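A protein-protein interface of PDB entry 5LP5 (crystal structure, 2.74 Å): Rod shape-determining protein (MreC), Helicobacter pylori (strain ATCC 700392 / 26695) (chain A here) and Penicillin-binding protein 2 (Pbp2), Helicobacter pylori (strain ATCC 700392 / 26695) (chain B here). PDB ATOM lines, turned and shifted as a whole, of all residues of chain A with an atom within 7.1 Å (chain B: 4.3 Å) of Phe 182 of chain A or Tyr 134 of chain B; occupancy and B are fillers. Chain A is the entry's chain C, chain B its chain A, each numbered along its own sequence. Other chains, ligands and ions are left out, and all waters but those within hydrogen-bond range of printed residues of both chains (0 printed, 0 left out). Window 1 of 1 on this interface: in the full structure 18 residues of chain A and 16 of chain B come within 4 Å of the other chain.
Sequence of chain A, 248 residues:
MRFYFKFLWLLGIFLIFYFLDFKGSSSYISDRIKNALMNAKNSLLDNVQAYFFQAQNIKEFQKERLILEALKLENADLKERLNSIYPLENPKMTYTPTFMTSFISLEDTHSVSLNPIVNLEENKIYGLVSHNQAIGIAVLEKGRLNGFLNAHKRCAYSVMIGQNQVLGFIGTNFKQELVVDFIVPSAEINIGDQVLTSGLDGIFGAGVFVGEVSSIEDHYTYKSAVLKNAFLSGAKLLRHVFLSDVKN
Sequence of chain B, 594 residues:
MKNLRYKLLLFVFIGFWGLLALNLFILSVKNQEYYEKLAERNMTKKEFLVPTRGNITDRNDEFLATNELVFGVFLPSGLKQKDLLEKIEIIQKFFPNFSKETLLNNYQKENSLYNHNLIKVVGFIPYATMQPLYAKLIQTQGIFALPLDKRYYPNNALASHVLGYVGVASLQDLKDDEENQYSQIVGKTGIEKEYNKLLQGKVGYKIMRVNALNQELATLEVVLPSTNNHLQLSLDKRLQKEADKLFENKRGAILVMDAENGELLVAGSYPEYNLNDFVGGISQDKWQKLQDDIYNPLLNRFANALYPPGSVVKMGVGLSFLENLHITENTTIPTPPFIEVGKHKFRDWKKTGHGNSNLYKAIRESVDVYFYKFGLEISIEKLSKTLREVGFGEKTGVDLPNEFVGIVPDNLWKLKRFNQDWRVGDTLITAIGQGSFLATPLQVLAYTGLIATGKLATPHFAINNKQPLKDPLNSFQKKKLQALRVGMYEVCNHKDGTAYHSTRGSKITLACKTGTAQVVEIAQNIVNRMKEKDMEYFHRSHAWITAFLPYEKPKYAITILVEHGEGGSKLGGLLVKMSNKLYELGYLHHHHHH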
ATOM      1  N   ILE A 125      -1.501  35.329   5.686  1.00  0.00           N
ATOM      2  CA  ILE A 125      -0.905  34.640   4.557  1.00  0.00           C
ATOM      3  C   ILE A 125      -0.194  35.619   3.624  1.00  0.00           C
ATOM      4  O   ILE A 125      -0.828  36.490   3.029  1.00  0.00           O
ATOM      5  CB  ILE A 125      -1.968  33.899   3.740  1.00  0.00           C
ATOM      6  CG1 ILE A 125      -2.698  32.878   4.599  1.00  0.00           C
ATOM      7  CG2 ILE A 125      -1.338  33.220   2.544  1.00  0.00           C
ATOM      8  CD1 ILE A 125      -4.067  32.526   4.061  1.00  0.00           C
ATOM      9  N   CYS A 155      -0.820  25.663  -0.328  1.00  0.00           N
ATOM     10  CA  CYS A 155      -0.532  26.798  -1.180  1.00  0.00           C
ATOM     11  C   CYS A 155      -1.707  27.069  -2.072  1.00  0.00           C
ATOM     12  O   CYS A 155      -2.058  26.239  -2.901  1.00  0.00           O
ATOM     13  CB  CYS A 155       0.717  26.548  -2.016  1.00  0.00           C
ATOM     14  SG  CYS A 155       0.955  27.804  -3.278  1.00  0.00           S
ATOM     15  N   ALA A 156      -2.319  28.231  -1.887  1.00  0.00           N
ATOM     16  CA  ALA A 156      -3.457  28.663  -2.694  1.00  0.00           C
ATOM     17  C   ALA A 156      -3.523  30.181  -2.750  1.00  0.00           C
ATOM     18  O   ALA A 156      -3.234  30.858  -1.779  1.00  0.00           O
ATOM     19  CB  ALA A 156      -4.759  28.114  -2.126  1.00  0.00           C
ATOM     20  N   TYR A 157      -3.896  30.717  -3.907  1.00  0.00           N
ATOM     21  CA  TYR A 157      -4.040  32.149  -4.050  1.00  0.00           C
ATOM     22  C   TYR A 157      -4.804  32.513  -5.308  1.00  0.00           C
ATOM     23  O   TYR A 157      -5.127  31.639  -6.093  1.00  0.00           O
ATOM     24  CB  TYR A 157      -2.685  32.824  -4.015  1.00  0.00           C
ATOM     25  CG  TYR A 157      -1.639  32.277  -4.961  1.00  0.00           C
ATOM     26  CD1 TYR A 157      -1.466  32.817  -6.223  1.00  0.00           C
ATOM     27  CD2 TYR A 157      -0.768  31.271  -4.563  1.00  0.00           C
ATOM     28  CE1 TYR A 157      -0.479  32.350  -7.087  1.00  0.00           C
ATOM     29  CE2 TYR A 157       0.229  30.806  -5.413  1.00  0.00           C
ATOM     30  CZ  TYR A 157       0.363  31.338  -6.671  1.00  0.00           C
ATOM     31  OH  TYR A 157       1.376  30.874  -7.482  1.00  0.00           O
ATOM     32  N   SER A 158      -5.152  33.795  -5.456  1.00  0.00           N
ATOM     33  CA  SER A 158      -6.029  34.259  -6.544  1.00  0.00           C
ATOM     34  C   SER A 158      -5.256  34.723  -7.770  1.00  0.00           C
ATOM     35  O   SER A 158      -4.390  35.573  -7.662  1.00  0.00           O
ATOM     36  CB  SER A 158      -6.924  35.396  -6.085  1.00  0.00           C
ATOM     37  OG  SER A 158      -7.845  35.679  -7.132  1.00  0.00           O
ATOM     38  N   LEU A 167     -10.900  34.934 -13.780  1.00  0.00           N
ATOM     39  CA  LEU A 167     -10.484  34.665 -12.405  1.00  0.00           C
ATOM     40  C   LEU A 167     -10.539  33.186 -12.061  1.00  0.00           C
ATOM     41  O   LEU A 167     -11.396  32.455 -12.554  1.00  0.00           O
ATOM     42  CB  LEU A 167     -11.388  35.433 -11.447  1.00  0.00           C
ATOM     43  CG  LEU A 167     -11.175  36.970 -11.450  1.00  0.00           C
ATOM     44  CD1 LEU A 167     -12.249  37.700 -10.645  1.00  0.00           C
ATOM     45  CD2 LEU A 167      -9.745  37.350 -10.985  1.00  0.00           C
ATOM     46  N   GLY A 168      -9.608  32.749 -11.229  1.00  0.00           N
ATOM     47  CA  GLY A 168      -9.616  31.397 -10.692  1.00  0.00           C
ATOM     48  C   GLY A 168      -8.795  31.356  -9.410  1.00  0.00           C
ATOM     49  O   GLY A 168      -8.321  32.398  -8.934  1.00  0.00           O
ATOM     50  N   PHE A 169      -8.636  30.158  -8.845  1.00  0.00           N
ATOM     51  CA  PHE A 169      -7.778  29.983  -7.665  1.00  0.00           C
ATOM     52  C   PHE A 169      -6.752  28.898  -7.864  1.00  0.00           C
ATOM     53  O   PHE A 169      -7.042  27.856  -8.462  1.00  0.00           O
ATOM     54  CB  PHE A 169      -8.592  29.654  -6.419  1.00  0.00           C
ATOM     55  CG  PHE A 169      -9.496  30.764  -5.969  1.00  0.00           C
ATOM     56  CD1 PHE A 169      -8.989  31.820  -5.221  1.00  0.00           C
ATOM     57  CD2 PHE A 169     -10.850  30.745  -6.273  1.00  0.00           C
ATOM     58  CE1 PHE A 169      -9.814  32.835  -4.793  1.00  0.00           C
ATOM     59  CE2 PHE A 169     -11.670  31.767  -5.856  1.00  0.00           C
ATOM     60  CZ  PHE A 169     -11.151  32.810  -5.107  1.00  0.00           C
ATOM     61  N   ILE A 170      -5.552  29.155  -7.372  1.00  0.00           N
ATOM     62  CA  ILE A 170      -4.454  28.238  -7.591  1.00  0.00           C
ATOM     63  C   ILE A 170      -4.642  27.045  -6.664  1.00  0.00           C
ATOM     64  O   ILE A 170      -4.904  27.178  -5.484  1.00  0.00           O
ATOM     65  CB  ILE A 170      -3.084  28.915  -7.343  1.00  0.00           C
ATOM     66  CG1 ILE A 170      -2.658  29.787  -8.536  1.00  0.00           C
ATOM     67  CG2 ILE A 170      -2.002  27.912  -7.001  1.00  0.00           C
ATOM     68  CD1 ILE A 170      -2.147  29.039  -9.748  1.00  0.00           C
ATOM     69  N   GLY A 171      -4.514  25.867  -7.239  1.00  0.00           N
ATOM     70  CA  GLY A 171      -4.389  24.658  -6.482  1.00  0.00           C
ATOM     71  C   GLY A 171      -3.378  23.771  -7.177  1.00  0.00           C
ATOM     72  O   GLY A 171      -2.423  24.243  -7.800  1.00  0.00           O
ATOM     73  N   VAL A 179      -2.287  24.169 -10.937  1.00  0.00           N
ATOM     74  CA  VAL A 179      -3.590  24.244 -11.606  1.00  0.00           C
ATOM     75  C   VAL A 179      -4.327  25.507 -11.216  1.00  0.00           C
ATOM     76  O   VAL A 179      -4.236  25.944 -10.070  1.00  0.00           O
ATOM     77  CB  VAL A 179      -4.450  23.036 -11.205  1.00  0.00           C
ATOM     78  CG1 VAL A 179      -5.869  23.188 -11.742  1.00  0.00           C
ATOM     79  CG2 VAL A 179      -3.777  21.725 -11.638  1.00  0.00           C
ATOM     80  N   VAL A 180      -5.029  26.109 -12.171  1.00  0.00           N
ATOM     81  CA  VAL A 180      -6.017  27.134 -11.836  1.00  0.00           C
ATOM     82  C   VAL A 180      -7.392  26.483 -11.830  1.00  0.00           C
ATOM     83  O   VAL A 180      -7.842  25.917 -12.825  1.00  0.00           O
ATOM     84  CB  VAL A 180      -6.026  28.311 -12.828  1.00  0.00           C
ATOM     85  CG1 VAL A 180      -7.067  29.333 -12.426  1.00  0.00           C
ATOM     86  CG2 VAL A 180      -4.652  28.956 -12.920  1.00  0.00           C
ATOM     87  N   ASP A 181      -8.058  26.587 -10.703  1.00  0.00           N
ATOM     88  CA  ASP A 181      -9.341  25.941 -10.483  1.00  0.00           C
ATOM     89  C   ASP A 181     -10.465  26.970 -10.438  1.00  0.00           C
ATOM     90  O   ASP A 181     -10.215  28.169 -10.272  1.00  0.00           O
ATOM     91  CB  ASP A 181      -9.275  25.178  -9.150  1.00  0.00           C
ATOM     92  CG  ASP A 181      -9.147  23.693  -9.337  1.00  0.00           C
ATOM     93  OD1 ASP A 181      -9.895  23.180 -10.204  1.00  0.00           O
ATOM     94  OD2 ASP A 181      -8.318  23.058  -8.626  1.00  0.00           O
ATOM     95  N   PHE A 182     -11.684  26.467 -10.608  1.00  0.00           N
ATOM     96  CA  PHE A 182     -12.922  27.221 -10.371  1.00  0.00           C
ATOM     97  C   PHE A 182     -13.209  28.384 -11.320  1.00  0.00           C
ATOM     98  O   PHE A 182     -13.752  29.407 -10.936  1.00  0.00           O
ATOM     99  CB  PHE A 182     -13.011  27.675  -8.917  1.00  0.00           C
ATOM    100  CG  PHE A 182     -12.692  26.594  -7.920  1.00  0.00           C
ATOM    101  CD1 PHE A 182     -13.264  25.321  -8.012  1.00  0.00           C
ATOM    102  CD2 PHE A 182     -11.742  26.834  -6.936  1.00  0.00           C
ATOM    103  CE1 PHE A 182     -12.929  24.338  -7.102  1.00  0.00           C
ATOM    104  CE2 PHE A 182     -11.429  25.860  -5.996  1.00  0.00           C
ATOM    105  CZ  PHE A 182     -12.023  24.610  -6.081  1.00  0.00           C
ATOM    106  N   ILE A 183     -12.906  28.171 -12.584  1.00  0.00           N
ATOM    107  CA  ILE A 183     -13.140  29.145 -13.648  1.00  0.00           C
ATOM    108  C   ILE A 183     -14.542  28.980 -14.239  1.00  0.00           C
ATOM    109  O   ILE A 183     -15.008  27.857 -14.468  1.00  0.00           O
ATOM    110  CB  ILE A 183     -12.139  28.917 -14.783  1.00  0.00           C
ATOM    111  CG1 ILE A 183     -10.712  28.882 -14.244  1.00  0.00           C
ATOM    112  CG2 ILE A 183     -12.268  29.959 -15.865  1.00  0.00           C
ATOM    113  CD1 ILE A 183      -9.694  28.286 -15.204  1.00  0.00           C
ATOM    114  N   VAL A 184     -15.194  30.093 -14.525  1.00  0.00           N
ATOM    115  CA  VAL A 184     -16.549  30.037 -15.096  1.00  0.00           C
ATOM    116  C   VAL A 184     -16.542  29.304 -16.428  1.00  0.00           C
ATOM    117  O   VAL A 184     -15.662  29.502 -17.229  1.00  0.00           O
ATOM    118  CB  VAL A 184     -17.191  31.448 -15.266  1.00  0.00           C
ATOM    119  CG1 VAL A 184     -17.316  32.165 -13.938  1.00  0.00           C
ATOM    120  CG2 VAL A 184     -16.367  32.317 -16.168  1.00  0.00           C
ATOM    121  N   PRO A 185     -17.534  28.451 -16.674  1.00  0.00           N
ATOM    122  CA  PRO A 185     -17.509  27.639 -17.890  1.00  0.00           C
ATOM    123  C   PRO A 185     -17.657  28.445 -19.185  1.00  0.00           C
ATOM    124  O   PRO A 185     -17.221  27.992 -20.243  1.00  0.00           O
ATOM    125  CB  PRO A 185     -18.710  26.687 -17.715  1.00  0.00           C
ATOM    126  CG  PRO A 185     -19.121  26.830 -16.295  1.00  0.00           C
ATOM    127  CD  PRO A 185     -18.767  28.235 -15.912  1.00  0.00           C
ATOM    128  N   ASP A 201      -6.721  38.942  -3.337  1.00  0.00           N
ATOM    129  CA  ASP A 201      -6.724  38.048  -2.178  1.00  0.00           C
ATOM    130  C   ASP A 201      -6.024  38.629  -0.947  1.00  0.00           C
ATOM    131  O   ASP A 201      -6.114  38.039   0.135  1.00  0.00           O
ATOM    132  CB  ASP A 201      -6.116  36.680  -2.550  1.00  0.00           C
ATOM    133  CG  ASP A 201      -4.752  36.791  -3.213  1.00  0.00           C
ATOM    134  OD1 ASP A 201      -4.187  37.888  -3.340  1.00  0.00           O
ATOM    135  OD2 ASP A 201      -4.231  35.758  -3.634  1.00  0.00           O
ATOM    136  N   HIS A 219     -15.178  20.570 -15.910  1.00  0.00           N
ATOM    137  CA  HIS A 219     -15.877  19.915 -14.804  1.00  0.00           C
ATOM    138  C   HIS A 219     -17.341  20.382 -14.734  1.00  0.00           C
ATOM    139  O   HIS A 219     -17.992  20.313 -13.689  1.00  0.00           O
ATOM    140  CB  HIS A 219     -15.209  20.209 -13.472  1.00  0.00           C
ATOM    141  CG  HIS A 219     -13.777  19.780 -13.387  1.00  0.00           C
ATOM    142  ND1 HIS A 219     -13.388  18.465 -13.241  1.00  0.00           N
ATOM    143  CD2 HIS A 219     -12.637  20.510 -13.396  1.00  0.00           C
ATOM    144  CE1 HIS A 219     -12.068  18.401 -13.200  1.00  0.00           C
ATOM    145  NE2 HIS A 219     -11.588  19.630 -13.284  1.00  0.00           N
ATOM    146  N   THR A 221     -19.654  22.544 -14.028  1.00  0.00           N
ATOM    147  CA  THR A 221     -20.074  23.770 -13.324  1.00  0.00           C
ATOM    148  C   THR A 221     -18.932  24.808 -13.310  1.00  0.00           C
ATOM    149  O   THR A 221     -19.127  25.986 -13.013  1.00  0.00           O
ATOM    150  CB  THR A 221     -20.604  23.507 -11.901  1.00  0.00           C
ATOM    151  OG1 THR A 221     -19.533  23.516 -10.957  1.00  0.00           O
ATOM    152  CG2 THR A 221     -21.345  22.162 -11.834  1.00  0.00           C
ATOM    153  N   TYR A 222     -17.745  24.345 -13.661  1.00  0.00           N
ATOM    154  CA  TYR A 222     -16.564  25.161 -13.735  1.00  0.00           C
ATOM    155  C   TYR A 222     -15.512  24.423 -14.576  1.00  0.00           C
ATOM    156  O   TYR A 222     -15.678  23.246 -14.905  1.00  0.00           O
ATOM    157  CB  TYR A 222     -16.045  25.424 -12.318  1.00  0.00           C
ATOM    158  CG  TYR A 222     -15.427  24.224 -11.643  1.00  0.00           C
ATOM    159  CD1 TYR A 222     -14.046  24.056 -11.612  1.00  0.00           C
ATOM    160  CD2 TYR A 222     -16.221  23.254 -11.035  1.00  0.00           C
ATOM    161  CE1 TYR A 222     -13.469  22.972 -10.976  1.00  0.00           C
ATOM    162  CE2 TYR A 222     -15.655  22.158 -10.392  1.00  0.00           C
ATOM    163  CZ  TYR A 222     -14.284  22.017 -10.381  1.00  0.00           C
ATOM    164  OH  TYR A 222     -13.730  20.931  -9.766  1.00  0.00           O
ATOM    165  N   LYS A 223     -14.438  25.136 -14.917  1.00  0.00           N
ATOM    166  CA  LYS A 223     -13.317  24.571 -15.649  1.00  0.00           C
ATOM    167  C   LYS A 223     -12.051  24.792 -14.879  1.00  0.00           C
ATOM    168  O   LYS A 223     -11.992  25.646 -14.013  1.00  0.00           O
ATOM    169  CB  LYS A 223     -13.145  25.289 -16.978  1.00  0.00           C
ATOM    170  CG  LYS A 223     -14.104  24.857 -18.074  1.00  0.00           C
ATOM    171  CD  LYS A 223     -13.834  25.602 -19.387  1.00  0.00           C
ATOM    172  CE  LYS A 223     -13.958  27.120 -19.250  1.00  0.00           C
ATOM    173  NZ  LYS A 223     -14.208  27.781 -20.554  1.00  0.00           N
ATOM    174  N   SER A 224     -11.029  24.023 -15.234  1.00  0.00           N
ATOM    175  CA  SER A 224      -9.705  24.159 -14.659  1.00  0.00           C
ATOM    176  C   SER A 224      -8.696  24.379 -15.768  1.00  0.00           C
ATOM    177  O   SER A 224      -8.933  24.012 -16.905  1.00  0.00           O
ATOM    178  CB  SER A 224      -9.313  22.881 -13.902  1.00  0.00           C
ATOM    179  OG  SER A 224     -10.034  22.707 -12.696  1.00  0.00           O
ATOM    180  N   ALA A 225      -7.560  24.955 -15.411  1.00  0.00           N
ATOM    181  CA  ALA A 225      -6.480  25.167 -16.346  1.00  0.00           C
ATOM    182  C   ALA A 225      -5.203  24.680 -15.728  1.00  0.00           C
ATOM    183  O   ALA A 225      -4.818  25.118 -14.649  1.00  0.00           O
ATOM    184  CB  ALA A 225      -6.346  26.646 -16.694  1.00  0.00           C
ATOM    185  N   LEU B  69     -21.697  30.975 -10.969  1.00  0.00           N
ATOM    186  CA  LEU B  69     -20.781  30.185 -10.187  1.00  0.00           C
ATOM    187  C   LEU B  69     -20.553  30.844  -8.836  1.00  0.00           C
ATOM    188  O   LEU B  69     -20.075  31.959  -8.734  1.00  0.00           O
ATOM    189  CB  LEU B  69     -19.477  30.033 -10.947  1.00  0.00           C
ATOM    190  CG  LEU B  69     -18.437  29.128 -10.342  1.00  0.00           C
ATOM    191  CD1 LEU B  69     -19.032  27.784  -9.957  1.00  0.00           C
ATOM    192  CD2 LEU B  69     -17.297  28.945 -11.341  1.00  0.00           C
ATOM    193  N   PHE B  71     -20.086  29.843  -4.266  1.00  0.00           N
ATOM    194  CA  PHE B  71     -19.395  28.937  -3.367  1.00  0.00           C
ATOM    195  C   PHE B  71     -20.260  28.446  -2.218  1.00  0.00           C
ATOM    196  O   PHE B  71     -21.409  28.843  -2.073  1.00  0.00           O
ATOM    197  CB  PHE B  71     -18.119  29.593  -2.852  1.00  0.00           C
ATOM    198  CG  PHE B  71     -16.989  29.519  -3.828  1.00  0.00           C
ATOM    199  CD1 PHE B  71     -16.216  28.375  -3.928  1.00  0.00           C
ATOM    200  CD2 PHE B  71     -16.716  30.579  -4.665  1.00  0.00           C
ATOM    201  CE1 PHE B  71     -15.184  28.304  -4.835  1.00  0.00           C
ATOM    202  CE2 PHE B  71     -15.682  30.510  -5.561  1.00  0.00           C
ATOM    203  CZ  PHE B  71     -14.916  29.378  -5.652  1.00  0.00           C
ATOM    204  N   TYR B 127     -18.640  34.977  -5.637  1.00  0.00           N
ATOM    205  CA  TYR B 127     -17.262  34.693  -5.999  1.00  0.00           C
ATOM    206  C   TYR B 127     -16.377  35.755  -5.355  1.00  0.00           C
ATOM    207  O   TYR B 127     -15.337  35.443  -4.797  1.00  0.00           O
ATOM    208  CB  TYR B 127     -17.113  34.676  -7.520  1.00  0.00           C
ATOM    209  CG  TYR B 127     -16.017  33.793  -8.052  1.00  0.00           C
ATOM    210  CD1 TYR B 127     -16.306  32.576  -8.624  1.00  0.00           C
ATOM    211  CD2 TYR B 127     -14.693  34.204  -8.027  1.00  0.00           C
ATOM    212  CE1 TYR B 127     -15.307  31.763  -9.124  1.00  0.00           C
ATOM    213  CE2 TYR B 127     -13.679  33.408  -8.526  1.00  0.00           C
ATOM    214  CZ  TYR B 127     -13.991  32.182  -9.067  1.00  0.00           C
ATOM    215  OH  TYR B 127     -12.993  31.364  -9.559  1.00  0.00           O
ATOM    216  N   MET B 130     -15.533  35.397  -1.779  1.00  0.00           N
ATOM    217  CA  MET B 130     -14.642  34.267  -1.530  1.00  0.00           C
ATOM    218  C   MET B 130     -13.183  34.669  -1.810  1.00  0.00           C
ATOM    219  O   MET B 130     -12.222  34.023  -1.387  1.00  0.00           O
ATOM    220  CB  MET B 130     -15.064  33.098  -2.429  1.00  0.00           C
ATOM    221  CG  MET B 130     -14.221  31.832  -2.275  1.00  0.00           C
ATOM    222  SD  MET B 130     -14.120  31.129  -0.609  1.00  0.00           S
ATOM    223  CE  MET B 130     -15.802  30.558  -0.516  1.00  0.00           C
ATOM    224  N   PRO B 132     -10.942  36.974  -0.804  1.00  0.00           N
ATOM    225  CA  PRO B 132      -9.979  36.969   0.312  1.00  0.00           C
ATOM    226  C   PRO B 132     -10.072  35.752   1.244  1.00  0.00           C
ATOM    227  O   PRO B 132      -9.164  35.515   2.012  1.00  0.00           O
ATOM    228  CB  PRO B 132     -10.327  38.232   1.086  1.00  0.00           C
ATOM    229  CG  PRO B 132     -11.750  38.537   0.746  1.00  0.00           C
ATOM    230  CD  PRO B 132     -12.102  37.831  -0.525  1.00  0.00           C
ATOM    231  N   LEU B 133     -11.153  34.990   1.158  1.00  0.00           N
ATOM    232  CA  LEU B 133     -11.385  33.851   2.047  1.00  0.00           C
ATOM    233  C   LEU B 133     -10.812  32.527   1.565  1.00  0.00           C
ATOM    234  O   LEU B 133     -10.394  31.732   2.369  1.00  0.00           O
ATOM    235  CB  LEU B 133     -12.887  33.650   2.272  1.00  0.00           C
ATOM    236  CG  LEU B 133     -13.673  34.873   2.745  1.00  0.00           C
ATOM    237  CD1 LEU B 133     -15.167  34.640   2.628  1.00  0.00           C
ATOM    238  CD2 LEU B 133     -13.301  35.231   4.165  1.00  0.00           C
ATOM    239  N   TYR B 134     -10.798  32.274   0.263  1.00  0.00           N
ATOM    240  CA  TYR B 134     -10.440  30.938  -0.211  1.00  0.00           C
ATOM    241  C   TYR B 134      -9.134  30.445   0.417  1.00  0.00           C
ATOM    242  O   TYR B 134      -9.079  29.364   0.952  1.00  0.00           O
ATOM    243  CB  TYR B 134     -10.371  30.859  -1.726  1.00  0.00           C
ATOM    244  CG  TYR B 134     -10.022  29.482  -2.225  1.00  0.00           C
ATOM    245  CD1 TYR B 134     -11.003  28.564  -2.507  1.00  0.00           C
ATOM    246  CD2 TYR B 134      -8.703  29.090  -2.420  1.00  0.00           C
ATOM    247  CE1 TYR B 134     -10.689  27.281  -2.955  1.00  0.00           C
ATOM    248  CE2 TYR B 134      -8.394  27.818  -2.863  1.00  0.00           C
ATOM    249  CZ  TYR B 134      -9.390  26.932  -3.121  1.00  0.00           C
ATOM    250  OH  TYR B 134      -9.064  25.693  -3.563  1.00  0.00           O
ATOM    251  N   ALA B 135      -8.086  31.234   0.383  1.00  0.00           N
ATOM    252  CA  ALA B 135      -6.795  30.800   0.945  1.00  0.00           C
ATOM    253  C   ALA B 135      -6.812  30.517   2.451  1.00  0.00           C
ATOM    254  O   ALA B 135      -6.120  29.624   2.944  1.00  0.00           O
ATOM    255  CB  ALA B 135      -5.717  31.833   0.630  1.00  0.00           C
ATOM    256  N   LYS B 136      -7.589  31.295   3.189  1.00  0.00           N
ATOM    257  CA  LYS B 136      -7.664  31.124   4.625  1.00  0.00           C
ATOM    258  C   LYS B 136      -8.431  29.863   4.984  1.00  0.00           C
ATOM    259  O   LYS B 136      -8.066  29.160   5.929  1.00  0.00           O
ATOM    260  CB  LYS B 136      -8.263  32.370   5.251  1.00  0.00           C
ATOM    261  CG  LYS B 136      -7.354  33.569   5.035  1.00  0.00           C
ATOM    262  CD  LYS B 136      -7.652  34.760   5.944  1.00  0.00           C
ATOM    263  CE  LYS B 136      -8.753  35.646   5.383  1.00  0.00           C
ATOM    264  NZ  LYS B 136      -9.649  36.182   6.460  1.00  0.00           N
ATOM    265  N   LEU B 137      -9.470  29.548   4.218  1.00  0.00           N
ATOM    266  CA  LEU B 137     -10.204  28.299   4.400  1.00  0.00           C
ATOM    267  C   LEU B 137      -9.334  27.070   4.109  1.00  0.00           C
ATOM    268  O   LEU B 137      -9.464  26.036   4.749  1.00  0.00           O
ATOM    269  CB  LEU B 137     -11.461  28.284   3.529  1.00  0.00           C
ATOM    270  CG  LEU B 137     -12.719  28.880   4.186  1.00  0.00           C
ATOM    271  CD1 LEU B 137     -12.492  30.330   4.589  1.00  0.00           C
ATOM    272  CD2 LEU B 137     -13.929  28.776   3.272  1.00  0.00           C
ATOM    273  N   ILE B 138      -8.421  27.202   3.168  1.00  0.00           N
ATOM    274  CA  ILE B 138      -7.530  26.119   2.783  1.00  0.00           C
ATOM    275  C   ILE B 138      -6.510  25.774   3.862  1.00  0.00           C
ATOM    276  O   ILE B 138      -5.983  24.682   3.872  1.00  0.00           O
ATOM    277  CB  ILE B 138      -6.820  26.470   1.444  1.00  0.00           C
ATOM    278  CG1 ILE B 138      -7.764  26.229   0.274  1.00  0.00           C
ATOM    279  CG2 ILE B 138      -5.530  25.688   1.233  1.00  0.00           C
ATOM    280  CD1 ILE B 138      -8.398  24.850   0.301  1.00  0.00           C
ATOM    281  N   PRO B 147     -17.395  24.780  -5.256  1.00  0.00           N
ATOM    282  CA  PRO B 147     -18.164  25.484  -6.277  1.00  0.00           C
ATOM    283  C   PRO B 147     -19.564  24.907  -6.460  1.00  0.00           C
ATOM    284  O   PRO B 147     -19.729  23.690  -6.570  1.00  0.00           O
ATOM    285  CB  PRO B 147     -17.331  25.268  -7.537  1.00  0.00           C
ATOM    286  CG  PRO B 147     -16.672  23.960  -7.314  1.00  0.00           C
ATOM    287  CD  PRO B 147     -16.424  23.842  -5.841  1.00  0.00           C
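SD of Met 130 of chain B sits at hydrogen-bond distance from N of Tyr 134 of chain B, at 3.6 Å. The backbone carbonyl oxygen (O) of Phe 169 of chain A is in hydrogen-bond range of the backbone NH (N) of Asp 181 of chain A. O of Ile 183 of chain A is in hydrogen-bond range of N of Lys 223 of chain A (2.8 Å).
Of the 12 printed residues of chain B, 6 touch a printed residue of chain A. Hydrophobic or aromatic side chains of chain A within 4 Å of the printed part of chain B: Ile 125, Ala 156, Phe 169, Phe 182 and Tyr 222. Along chain A the printed residues that touch a printed residue of chain B span positions 125 to 222. Among the printed residues, 17 pairs touch across the chains. Among the printed residues, no Asp or Glu carboxylate lies within 4 Å of a Lys or Arg side-chain nitrogen of the other chain.
The side-chain hydroxyl (OH) of Tyr 127 of chain B is in hydrogen-bond range of the backbone carbonyl oxygen (O) of Phe 182 of chain A (2.5 Å).
Among the printed residues, merely in contact across the chains: Phe 182 of chain A with Tyr 134 of chain B (3.4 Å), Thr 221 of chain A with Leu 69 of chain B (3.5 Å), Gly 168 of chain A with Tyr 127 of chain B (3.6 Å), Leu 167 of chain A with Tyr 127 of chain B (3.6 Å), Ile 125 of chain A with Lys 136 of chain B (3.6 Å), Ala 156 of chain A with Ala 135 of chain B (3.6 Å), Phe 182 of chain A with Leu 69 of chain B (3.6 Å), Phe 169 of chain A with Tyr 134 of chain B (3.7 Å), Tyr 222 of chain A with Pro 147 of chain B (3.7 Å), Ala 156 of chain A with Tyr 134 of chain B (3.7 Å), Phe 169 of chain A with Tyr 127 of chain B (3.7 Å), Ile 125 of chain A with Ala 135 of chain B (3.7 Å), Phe 182 of chain A with Pro 147 of chain B (3.7 Å), Tyr 222 of chain A with Leu 69 of chain B (3.9 Å), Val 184 of chain A with Leu 69 of chain B (3.98 Å) and Ile 183 of chain A with Leu 69 of chain B (3.999 Å).
Printed residues of chain B within 4 Å of Ile 125 of chain A: Ala 135 and Lys 136. Printed residues of chain A within 4 Å of Lys 136 of chain B: Ile 125 (3.6 Å). The nearest printed residue of chain B that does not touch Gly 168 of chain A is Tyr 134 of chain B (7.3 Å).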
